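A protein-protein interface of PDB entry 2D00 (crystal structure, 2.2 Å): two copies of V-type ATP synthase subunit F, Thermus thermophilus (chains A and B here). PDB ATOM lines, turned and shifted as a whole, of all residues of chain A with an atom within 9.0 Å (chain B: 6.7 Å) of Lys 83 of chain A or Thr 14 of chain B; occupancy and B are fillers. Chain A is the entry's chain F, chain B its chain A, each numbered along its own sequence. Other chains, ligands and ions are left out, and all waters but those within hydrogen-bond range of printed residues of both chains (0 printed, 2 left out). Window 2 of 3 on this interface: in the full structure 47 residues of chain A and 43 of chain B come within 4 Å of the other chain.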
ATOM      1  N   ILE A  79     -33.005  31.433  13.301  1.00  0.00           N
ATOM      2  CA  ILE A  79     -32.153  32.406  14.086  1.00  0.00           C
ATOM      3  C   ILE A  79     -30.680  32.092  13.913  1.00  0.00           C
ATOM      4  O   ILE A  79     -30.242  30.915  14.033  1.00  0.00           O
ATOM      5  CB  ILE A  79     -32.397  32.274  15.595  1.00  0.00           C
ATOM      6  CG1 ILE A  79     -33.870  32.326  15.972  1.00  0.00           C
ATOM      7  CG2 ILE A  79     -31.706  33.332  16.309  1.00  0.00           C
ATOM      8  CD1 ILE A  79     -34.403  33.727  15.622  1.00  0.00           C
ATOM      9  N   ALA A  80     -29.924  33.158  13.740  1.00  0.00           N
ATOM     10  CA  ALA A  80     -28.466  33.164  13.788  1.00  0.00           C
ATOM     11  C   ALA A  80     -27.964  33.415  15.217  1.00  0.00           C
ATOM     12  O   ALA A  80     -28.468  34.307  15.916  1.00  0.00           O
ATOM     13  CB  ALA A  80     -27.951  34.168  12.858  1.00  0.00           C
ATOM     14  N   GLY A  81     -27.054  32.542  15.683  1.00  0.00           N
ATOM     15  CA  GLY A  81     -26.420  32.721  16.993  1.00  0.00           C
ATOM     16  C   GLY A  81     -27.265  32.424  18.220  1.00  0.00           C
ATOM     17  O   GLY A  81     -27.307  33.218  19.163  1.00  0.00           O
ATOM     18  N   LEU A  82     -27.944  31.293  18.231  1.00  0.00           N
ATOM     19  CA  LEU A  82     -28.581  30.819  19.466  1.00  0.00           C
ATOM     20  C   LEU A  82     -27.563  30.418  20.564  1.00  0.00           C
ATOM     21  O   LEU A  82     -27.881  30.483  21.766  1.00  0.00           O
ATOM     22  CB  LEU A  82     -29.464  29.577  19.168  1.00  0.00           C
ATOM     23  CG  LEU A  82     -30.722  29.841  18.409  1.00  0.00           C
ATOM     24  CD1 LEU A  82     -31.541  28.553  18.093  1.00  0.00           C
ATOM     25  CD2 LEU A  82     -31.599  30.792  19.208  1.00  0.00           C
ATOM     26  N   LYS A  83     -26.395  29.931  20.138  1.00  0.00           N
ATOM     27  CA  LYS A  83     -25.321  29.606  21.060  1.00  0.00           C
ATOM     28  C   LYS A  83     -24.996  30.812  21.947  1.00  0.00           C
ATOM     29  O   LYS A  83     -24.624  30.693  23.099  1.00  0.00           O
ATOM     30  CB  LYS A  83     -24.069  29.213  20.279  1.00  0.00           C
ATOM     31  CG  LYS A  83     -24.229  27.953  19.507  1.00  0.00           C
ATOM     32  CD  LYS A  83     -23.195  27.927  18.374  1.00  0.00           C
ATOM     33  CE  LYS A  83     -23.830  27.379  17.102  1.00  0.00           C
ATOM     34  NZ  LYS A  83     -24.157  25.952  17.202  1.00  0.00           N
ATOM     35  N   GLU A  84     -25.152  31.985  21.367  1.00  0.00           N
ATOM     36  CA  GLU A  84     -24.735  33.188  22.001  1.00  0.00           C
ATOM     37  C   GLU A  84     -25.653  33.589  23.149  1.00  0.00           C
ATOM     38  O   GLU A  84     -25.334  34.534  23.872  1.00  0.00           O
ATOM     39  CB  GLU A  84     -24.697  34.283  20.980  1.00  0.00           C
ATOM     40  CG  GLU A  84     -23.699  34.123  19.886  1.00  0.00           C
ATOM     41  CD  GLU A  84     -23.424  35.509  19.290  1.00  0.00           C
ATOM     42  OE1 GLU A  84     -24.411  36.075  18.694  1.00  0.00           O
ATOM     43  OE2 GLU A  84     -22.272  36.065  19.493  1.00  0.00           O
ATOM     44  N   ALA A  85     -26.751  32.867  23.346  1.00  0.00           N
ATOM     45  CA  ALA A  85     -27.700  33.155  24.426  1.00  0.00           C
ATOM     46  C   ALA A  85     -27.289  32.642  25.837  1.00  0.00           C
ATOM     47  O   ALA A  85     -27.927  32.977  26.844  1.00  0.00           O
ATOM     48  CB  ALA A  85     -29.029  32.659  24.066  1.00  0.00           C
ATOM     49  N   PHE A  86     -26.204  31.868  25.914  1.00  0.00           N
ATOM     50  CA  PHE A  86     -25.740  31.311  27.168  1.00  0.00           C
ATOM     51  C   PHE A  86     -24.611  32.184  27.573  1.00  0.00           C
ATOM     52  O   PHE A  86     -24.406  32.449  28.789  1.00  0.00           O
ATOM     53  CB  PHE A  86     -25.183  29.885  27.030  1.00  0.00           C
ATOM     54  CG  PHE A  86     -26.059  28.932  26.284  1.00  0.00           C
ATOM     55  CD1 PHE A  86     -25.511  28.016  25.420  1.00  0.00           C
ATOM     56  CD2 PHE A  86     -27.429  28.955  26.412  1.00  0.00           C
ATOM     57  CE1 PHE A  86     -26.318  27.166  24.763  1.00  0.00           C
ATOM     58  CE2 PHE A  86     -28.182  28.137  25.752  1.00  0.00           C
ATOM     59  CZ  PHE A  86     -27.660  27.273  24.932  1.00  0.00           C
ATOM     60  N   GLN A  87     -23.852  32.616  26.555  1.00  0.00           N
ATOM     61  CA  GLN A  87     -22.661  33.424  26.791  1.00  0.00           C
ATOM     62  C   GLN A  87     -23.075  34.826  27.171  1.00  0.00           C
ATOM     63  O   GLN A  87     -22.242  35.682  27.207  1.00  0.00           O
ATOM     64  CB  GLN A  87     -21.631  33.381  25.631  1.00  0.00           C
ATOM     65  CG  GLN A  87     -21.762  34.444  24.545  1.00  0.00           C
ATOM     66  CD  GLN A  87     -20.808  34.197  23.364  1.00  0.00           C
ATOM     67  OE1 GLN A  87     -19.986  35.051  23.025  1.00  0.00           O
ATOM     68  NE2 GLN A  87     -20.922  33.025  22.735  1.00  0.00           N
ATOM     69  N   GLY A  88     -24.373  35.025  27.437  1.00  0.00           N
ATOM     70  CA  GLY A  88     -24.849  36.034  28.401  1.00  0.00           C
ATOM     71  C   GLY A  88     -24.835  35.467  29.829  1.00  0.00           C
ATOM     72  O   GLY A  88     -23.833  34.880  30.253  1.00  0.00           O
ATOM     73  N   VAL A  91     -30.454  33.470  29.705  1.00  0.00           N
ATOM     74  CA  VAL A  91     -30.970  32.926  28.429  1.00  0.00           C
ATOM     75  C   VAL A  91     -32.416  33.318  28.166  1.00  0.00           C
ATOM     76  O   VAL A  91     -32.767  33.736  27.054  1.00  0.00           O
ATOM     77  CB  VAL A  91     -30.857  31.383  28.403  1.00  0.00           C
ATOM     78  CG1 VAL A  91     -31.405  30.787  27.108  1.00  0.00           C
ATOM     79  CG2 VAL A  91     -29.426  30.975  28.601  1.00  0.00           C
ATOM     80  N   TYR A  94     -32.498  37.128  27.197  1.00  0.00           N
ATOM     81  CA  TYR A  94     -31.821  37.222  25.927  1.00  0.00           C
ATOM     82  C   TYR A  94     -32.724  36.680  24.796  1.00  0.00           C
ATOM     83  O   TYR A  94     -32.711  37.182  23.679  1.00  0.00           O
ATOM     84  CB  TYR A  94     -30.529  36.432  25.978  1.00  0.00           C
ATOM     85  CG  TYR A  94     -29.801  36.377  24.653  1.00  0.00           C
ATOM     86  CD1 TYR A  94     -28.697  37.207  24.406  1.00  0.00           C
ATOM     87  CD2 TYR A  94     -30.211  35.517  23.647  1.00  0.00           C
ATOM     88  CE1 TYR A  94     -28.027  37.188  23.187  1.00  0.00           C
ATOM     89  CE2 TYR A  94     -29.536  35.478  22.428  1.00  0.00           C
ATOM     90  CZ  TYR A  94     -28.442  36.330  22.217  1.00  0.00           C
ATOM     91  OH  TYR A  94     -27.758  36.279  21.032  1.00  0.00           O
ATOM     92  N   MET A  95     -33.522  35.676  25.102  1.00  0.00           N
ATOM     93  CA  MET A  95     -34.427  35.075  24.103  1.00  0.00           C
ATOM     94  C   MET A  95     -35.690  35.954  23.873  1.00  0.00           C
ATOM     95  O   MET A  95     -36.160  36.144  22.753  1.00  0.00           O
ATOM     96  CB  MET A  95     -34.762  33.649  24.574  1.00  0.00           C
ATOM     97  CG  MET A  95     -34.723  32.597  23.519  1.00  0.00           C
ATOM     98  SD  MET A  95     -33.254  32.417  22.463  1.00  0.00           S
ATOM     99  CE  MET A  95     -34.152  32.167  20.967  1.00  0.00           C
ATOM    100  N   LEU A  98     -34.367  38.694  21.663  1.00  0.00           N
ATOM    101  CA  LEU A  98     -34.048  38.244  20.319  1.00  0.00           C
ATOM    102  C   LEU A  98     -35.294  37.954  19.406  1.00  0.00           C
ATOM    103  O   LEU A  98     -35.256  38.202  18.200  1.00  0.00           O
ATOM    104  CB  LEU A  98     -33.180  36.997  20.422  1.00  0.00           C
ATOM    105  CG  LEU A  98     -32.162  36.849  19.298  1.00  0.00           C
ATOM    106  CD1 LEU A  98     -31.232  35.687  19.614  1.00  0.00           C
ATOM    107  CD2 LEU A  98     -32.882  36.660  17.950  1.00  0.00           C
ATOM    108  N   VAL B   8     -37.606  25.716  20.786  1.00  0.00           N
ATOM    109  CA  VAL B   8     -36.333  26.030  20.154  1.00  0.00           C
ATOM    110  C   VAL B   8     -35.716  24.823  19.562  1.00  0.00           C
ATOM    111  O   VAL B   8     -35.672  23.829  20.212  1.00  0.00           O
ATOM    112  CB  VAL B   8     -35.292  26.638  21.190  1.00  0.00           C
ATOM    113  CG1 VAL B   8     -34.115  27.159  20.501  1.00  0.00           C
ATOM    114  CG2 VAL B   8     -36.004  27.888  21.969  1.00  0.00           C
ATOM    115  N   ALA B  10     -32.295  23.290  17.924  1.00  0.00           N
ATOM    116  CA  ALA B  10     -30.921  23.628  17.767  1.00  0.00           C
ATOM    117  C   ALA B  10     -30.098  22.305  17.786  1.00  0.00           C
ATOM    118  O   ALA B  10     -30.646  21.242  17.917  1.00  0.00           O
ATOM    119  CB  ALA B  10     -30.504  24.598  18.850  1.00  0.00           C
ATOM    120  N   ASP B  11     -28.792  22.447  17.640  1.00  0.00           N
ATOM    121  CA  ASP B  11     -27.861  21.326  17.654  1.00  0.00           C
ATOM    122  C   ASP B  11     -27.999  20.767  19.059  1.00  0.00           C
ATOM    123  O   ASP B  11     -28.427  21.441  19.943  1.00  0.00           O
ATOM    124  CB  ASP B  11     -26.434  21.811  17.373  1.00  0.00           C
ATOM    125  CG  ASP B  11     -25.842  22.686  18.513  1.00  0.00           C
ATOM    126  OD1 ASP B  11     -25.921  23.970  18.417  1.00  0.00           O
ATOM    127  OD2 ASP B  11     -25.289  22.102  19.509  1.00  0.00           O
ATOM    128  N   PRO B  12     -27.745  19.493  19.226  1.00  0.00           N
ATOM    129  CA  PRO B  12     -27.992  18.883  20.548  1.00  0.00           C
ATOM    130  C   PRO B  12     -27.340  19.485  21.812  1.00  0.00           C
ATOM    131  O   PRO B  12     -27.927  19.492  22.871  1.00  0.00           O
ATOM    132  CB  PRO B  12     -27.602  17.429  20.350  1.00  0.00           C
ATOM    133  CG  PRO B  12     -27.661  17.165  18.811  1.00  0.00           C
ATOM    134  CD  PRO B  12     -27.367  18.529  18.170  1.00  0.00           C
ATOM    135  N   GLU B  13     -26.107  19.910  21.725  1.00  0.00           N
ATOM    136  CA  GLU B  13     -25.443  20.540  22.880  1.00  0.00           C
ATOM    137  C   GLU B  13     -26.194  21.798  23.309  1.00  0.00           C
ATOM    138  O   GLU B  13     -26.483  22.038  24.456  1.00  0.00           O
ATOM    139  CB  GLU B  13     -24.019  20.924  22.481  1.00  0.00           C
ATOM    140  CG  GLU B  13     -22.918  20.155  23.044  1.00  0.00           C
ATOM    141  CD  GLU B  13     -21.585  20.671  22.505  1.00  0.00           C
ATOM    142  OE1 GLU B  13     -20.518  20.336  23.108  1.00  0.00           O
ATOM    143  OE2 GLU B  13     -21.635  21.406  21.461  1.00  0.00           O
ATOM    144  N   THR B  14     -26.500  22.630  22.355  1.00  0.00           N
ATOM    145  CA  THR B  14     -27.250  23.889  22.610  1.00  0.00           C
ATOM    146  C   THR B  14     -28.638  23.649  23.140  1.00  0.00           C
ATOM    147  O   THR B  14     -29.115  24.335  24.082  1.00  0.00           O
ATOM    148  CB  THR B  14     -27.213  24.714  21.312  1.00  0.00           C
ATOM    149  OG1 THR B  14     -25.827  24.901  20.994  1.00  0.00           O
ATOM    150  CG2 THR B  14     -27.869  26.040  21.460  1.00  0.00           C
ATOM    151  N   ALA B  15     -29.278  22.658  22.537  1.00  0.00           N
ATOM    152  CA  ALA B  15     -30.655  22.289  22.899  1.00  0.00           C
ATOM    153  C   ALA B  15     -30.710  21.898  24.365  1.00  0.00           C
ATOM    154  O   ALA B  15     -31.582  22.314  25.061  1.00  0.00           O
ATOM    155  CB  ALA B  15     -31.068  21.111  22.061  1.00  0.00           C
ATOM    156  N   GLN B  16     -29.732  21.070  24.790  1.00  0.00           N
ATOM    157  CA  GLN B  16     -29.503  20.752  26.165  1.00  0.00           C
ATOM    158  C   GLN B  16     -29.362  21.957  27.056  1.00  0.00           C
ATOM    159  O   GLN B  16     -29.852  21.934  28.162  1.00  0.00           O
ATOM    160  CB  GLN B  16     -28.223  19.969  26.324  1.00  0.00           C
ATOM    161  CG  GLN B  16     -28.373  18.752  27.107  1.00  0.00           C
ATOM    162  CD  GLN B  16     -27.149  17.953  27.073  1.00  0.00           C
ATOM    163  OE1 GLN B  16     -26.083  18.486  26.778  1.00  0.00           O
ATOM    164  NE2 GLN B  16     -27.267  16.685  27.315  1.00  0.00           N
ATOM    165  N   GLY B  17     -28.598  22.943  26.607  1.00  0.00           N
ATOM    166  CA  GLY B  17     -28.432  24.202  27.377  1.00  0.00           C
ATOM    167  C   GLY B  17     -29.714  25.048  27.515  1.00  0.00           C
ATOM    168  O   GLY B  17     -29.935  25.701  28.514  1.00  0.00           O
ATOM    169  N   PHE B  18     -30.532  25.078  26.489  1.00  0.00           N
ATOM    170  CA  PHE B  18     -31.810  25.775  26.592  1.00  0.00           C
ATOM    171  C   PHE B  18     -32.675  25.066  27.613  1.00  0.00           C
ATOM    172  O   PHE B  18     -33.264  25.741  28.421  1.00  0.00           O
ATOM    173  CB  PHE B  18     -32.487  25.845  25.264  1.00  0.00           C
ATOM    174  CG  PHE B  18     -32.023  26.960  24.443  1.00  0.00           C
ATOM    175  CD1 PHE B  18     -31.177  26.776  23.407  1.00  0.00           C
ATOM    176  CD2 PHE B  18     -32.444  28.231  24.717  1.00  0.00           C
ATOM    177  CE1 PHE B  18     -30.745  27.826  22.630  1.00  0.00           C
ATOM    178  CE2 PHE B  18     -31.987  29.312  23.932  1.00  0.00           C
ATOM    179  CZ  PHE B  18     -31.114  29.087  22.912  1.00  0.00           C
ATOM    180  N   ARG B  19     -32.713  23.735  27.616  1.00  0.00           N
ATOM    181  CA  ARG B  19     -33.409  22.971  28.667  1.00  0.00           C
ATOM    182  C   ARG B  19     -32.994  23.267  30.144  1.00  0.00           C
ATOM    183  O   ARG B  19     -33.820  23.358  31.062  1.00  0.00           O
ATOM    184  CB  ARG B  19     -33.320  21.459  28.347  1.00  0.00           C
ATOM    185  CG  ARG B  19     -34.194  21.097  27.095  1.00  0.00           C
ATOM    186  CD  ARG B  19     -34.452  19.528  26.872  1.00  0.00           C
ATOM    187  NE  ARG B  19     -33.209  18.792  26.763  1.00  0.00           N
ATOM    188  CZ  ARG B  19     -32.520  18.551  25.641  1.00  0.00           C
ATOM    189  NH1 ARG B  19     -32.961  18.927  24.473  1.00  0.00           N
ATOM    190  NH2 ARG B  19     -31.378  17.879  25.697  1.00  0.00           N
ATOM    191  N   GLY B  25     -36.063  23.252  24.494  1.00  0.00           N
ATOM    192  CA  GLY B  25     -35.119  23.007  23.416  1.00  0.00           C
ATOM    193  C   GLY B  25     -35.212  21.558  23.014  1.00  0.00           C
ATOM    194  O   GLY B  25     -35.295  20.746  23.839  1.00  0.00           O
ATOM    195  N   ASP B  53     -32.445  27.221  14.795  1.00  0.00           N
ATOM    196  CA  ASP B  53     -31.132  27.583  14.301  1.00  0.00           C
ATOM    197  C   ASP B  53     -31.191  27.645  12.770  1.00  0.00           C
ATOM    198  O   ASP B  53     -31.647  26.672  12.134  1.00  0.00           O
ATOM    199  CB  ASP B  53     -30.187  26.427  14.642  1.00  0.00           C
ATOM    200  CG  ASP B  53     -28.745  26.852  14.602  1.00  0.00           C
ATOM    201  OD1 ASP B  53     -28.180  27.101  13.514  1.00  0.00           O
ATOM    202  OD2 ASP B  53     -28.217  27.022  15.691  1.00  0.00           O
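OD1 of Asp 11 of chain B lies within salt-bridge range of NZ of Lys 83 of chain A (2.9 Å).
N of Glu 13 of chain B sits at hydrogen-bond distance from OD2 of Asp 11 of chain B, 3.2 Å away.
OD1 of Asp 11 of chain B lies within hydrogen-bond range of OG1 of Thr 14 of chain B (2.7 Å).
Asp 53 of chain B touches Ile 79 of chain A.
CG1 of Val 8 of chain B touches CD1 of Leu 82 of chain A, at 3.8 Å.
Phe 18 of chain B touches Leu 82 of chain A (CZ to O, 3.7 Å).
Leu 82 of chain A touches Asp 53 of chain B (CD1 to N, 3.7 Å).
Thr 14 of chain B touches Lys 83 of chain A.
Phe 86 of chain A touches Thr 14 of chain B.
Phe 86 of chain A touches Gly 17 of chain B (CE2 to C, 3.9 Å).
Phe 86 of chain A touches Phe 18 of chain B.
Phe 18 of chain B touches Val 91 of chain A (CE2 to CG1, 3.5 Å).
Met 95 of chain A touches Phe 18 of chain B.
Of chain B, only Asp 11 (2.9 Å) and Thr 14 (3.8 Å) come within 4 Å of Lys 83 of chain A.
Thr 14 of chain B touches just these residues of chain A: Lys 83 (3.8 Å) and Phe 86 (3.4 Å).
No residue of chain A comes within 4 Å of Ala 15 of chain B.
Gly 17 of chain B touches just one residue of chain A: Phe 86.
Of the printed residues of chain A, Phe 18 of chain B touches Leu 82, Phe 86, Val 91 and Met 95.
Of the printed residues of chain A, Asp 53 of chain B touches Ile 79 and Leu 82.
Gly 88 of chain A touches none of the printed residues of chain B.
Arg 19 of chain B touches none of the printed residues of chain A.
The nearest printed residue of chain A that does not touch Asp 53 of chain B is Lys 83 of chain A (4.5 Å).
Of the 13 printed residues of chain B, 6 touch a printed residue of chain A.
Hydrophobic or aromatic side chains of chain A that line the printed part of chain B: Leu 82, Phe 86, Val 91 and Met 95.
Among the printed residues, Asp or Glu carboxylates within 4 Å of a Lys or Arg side-chain nitrogen of the other chain: Lys 83 of chain A with Asp 11 of chain B (2.9 Å).
No position is printed for both chains.
Of the 11 pairs that touch across the chains among the printed residues, none has its exchanged pair printed and touching as well.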
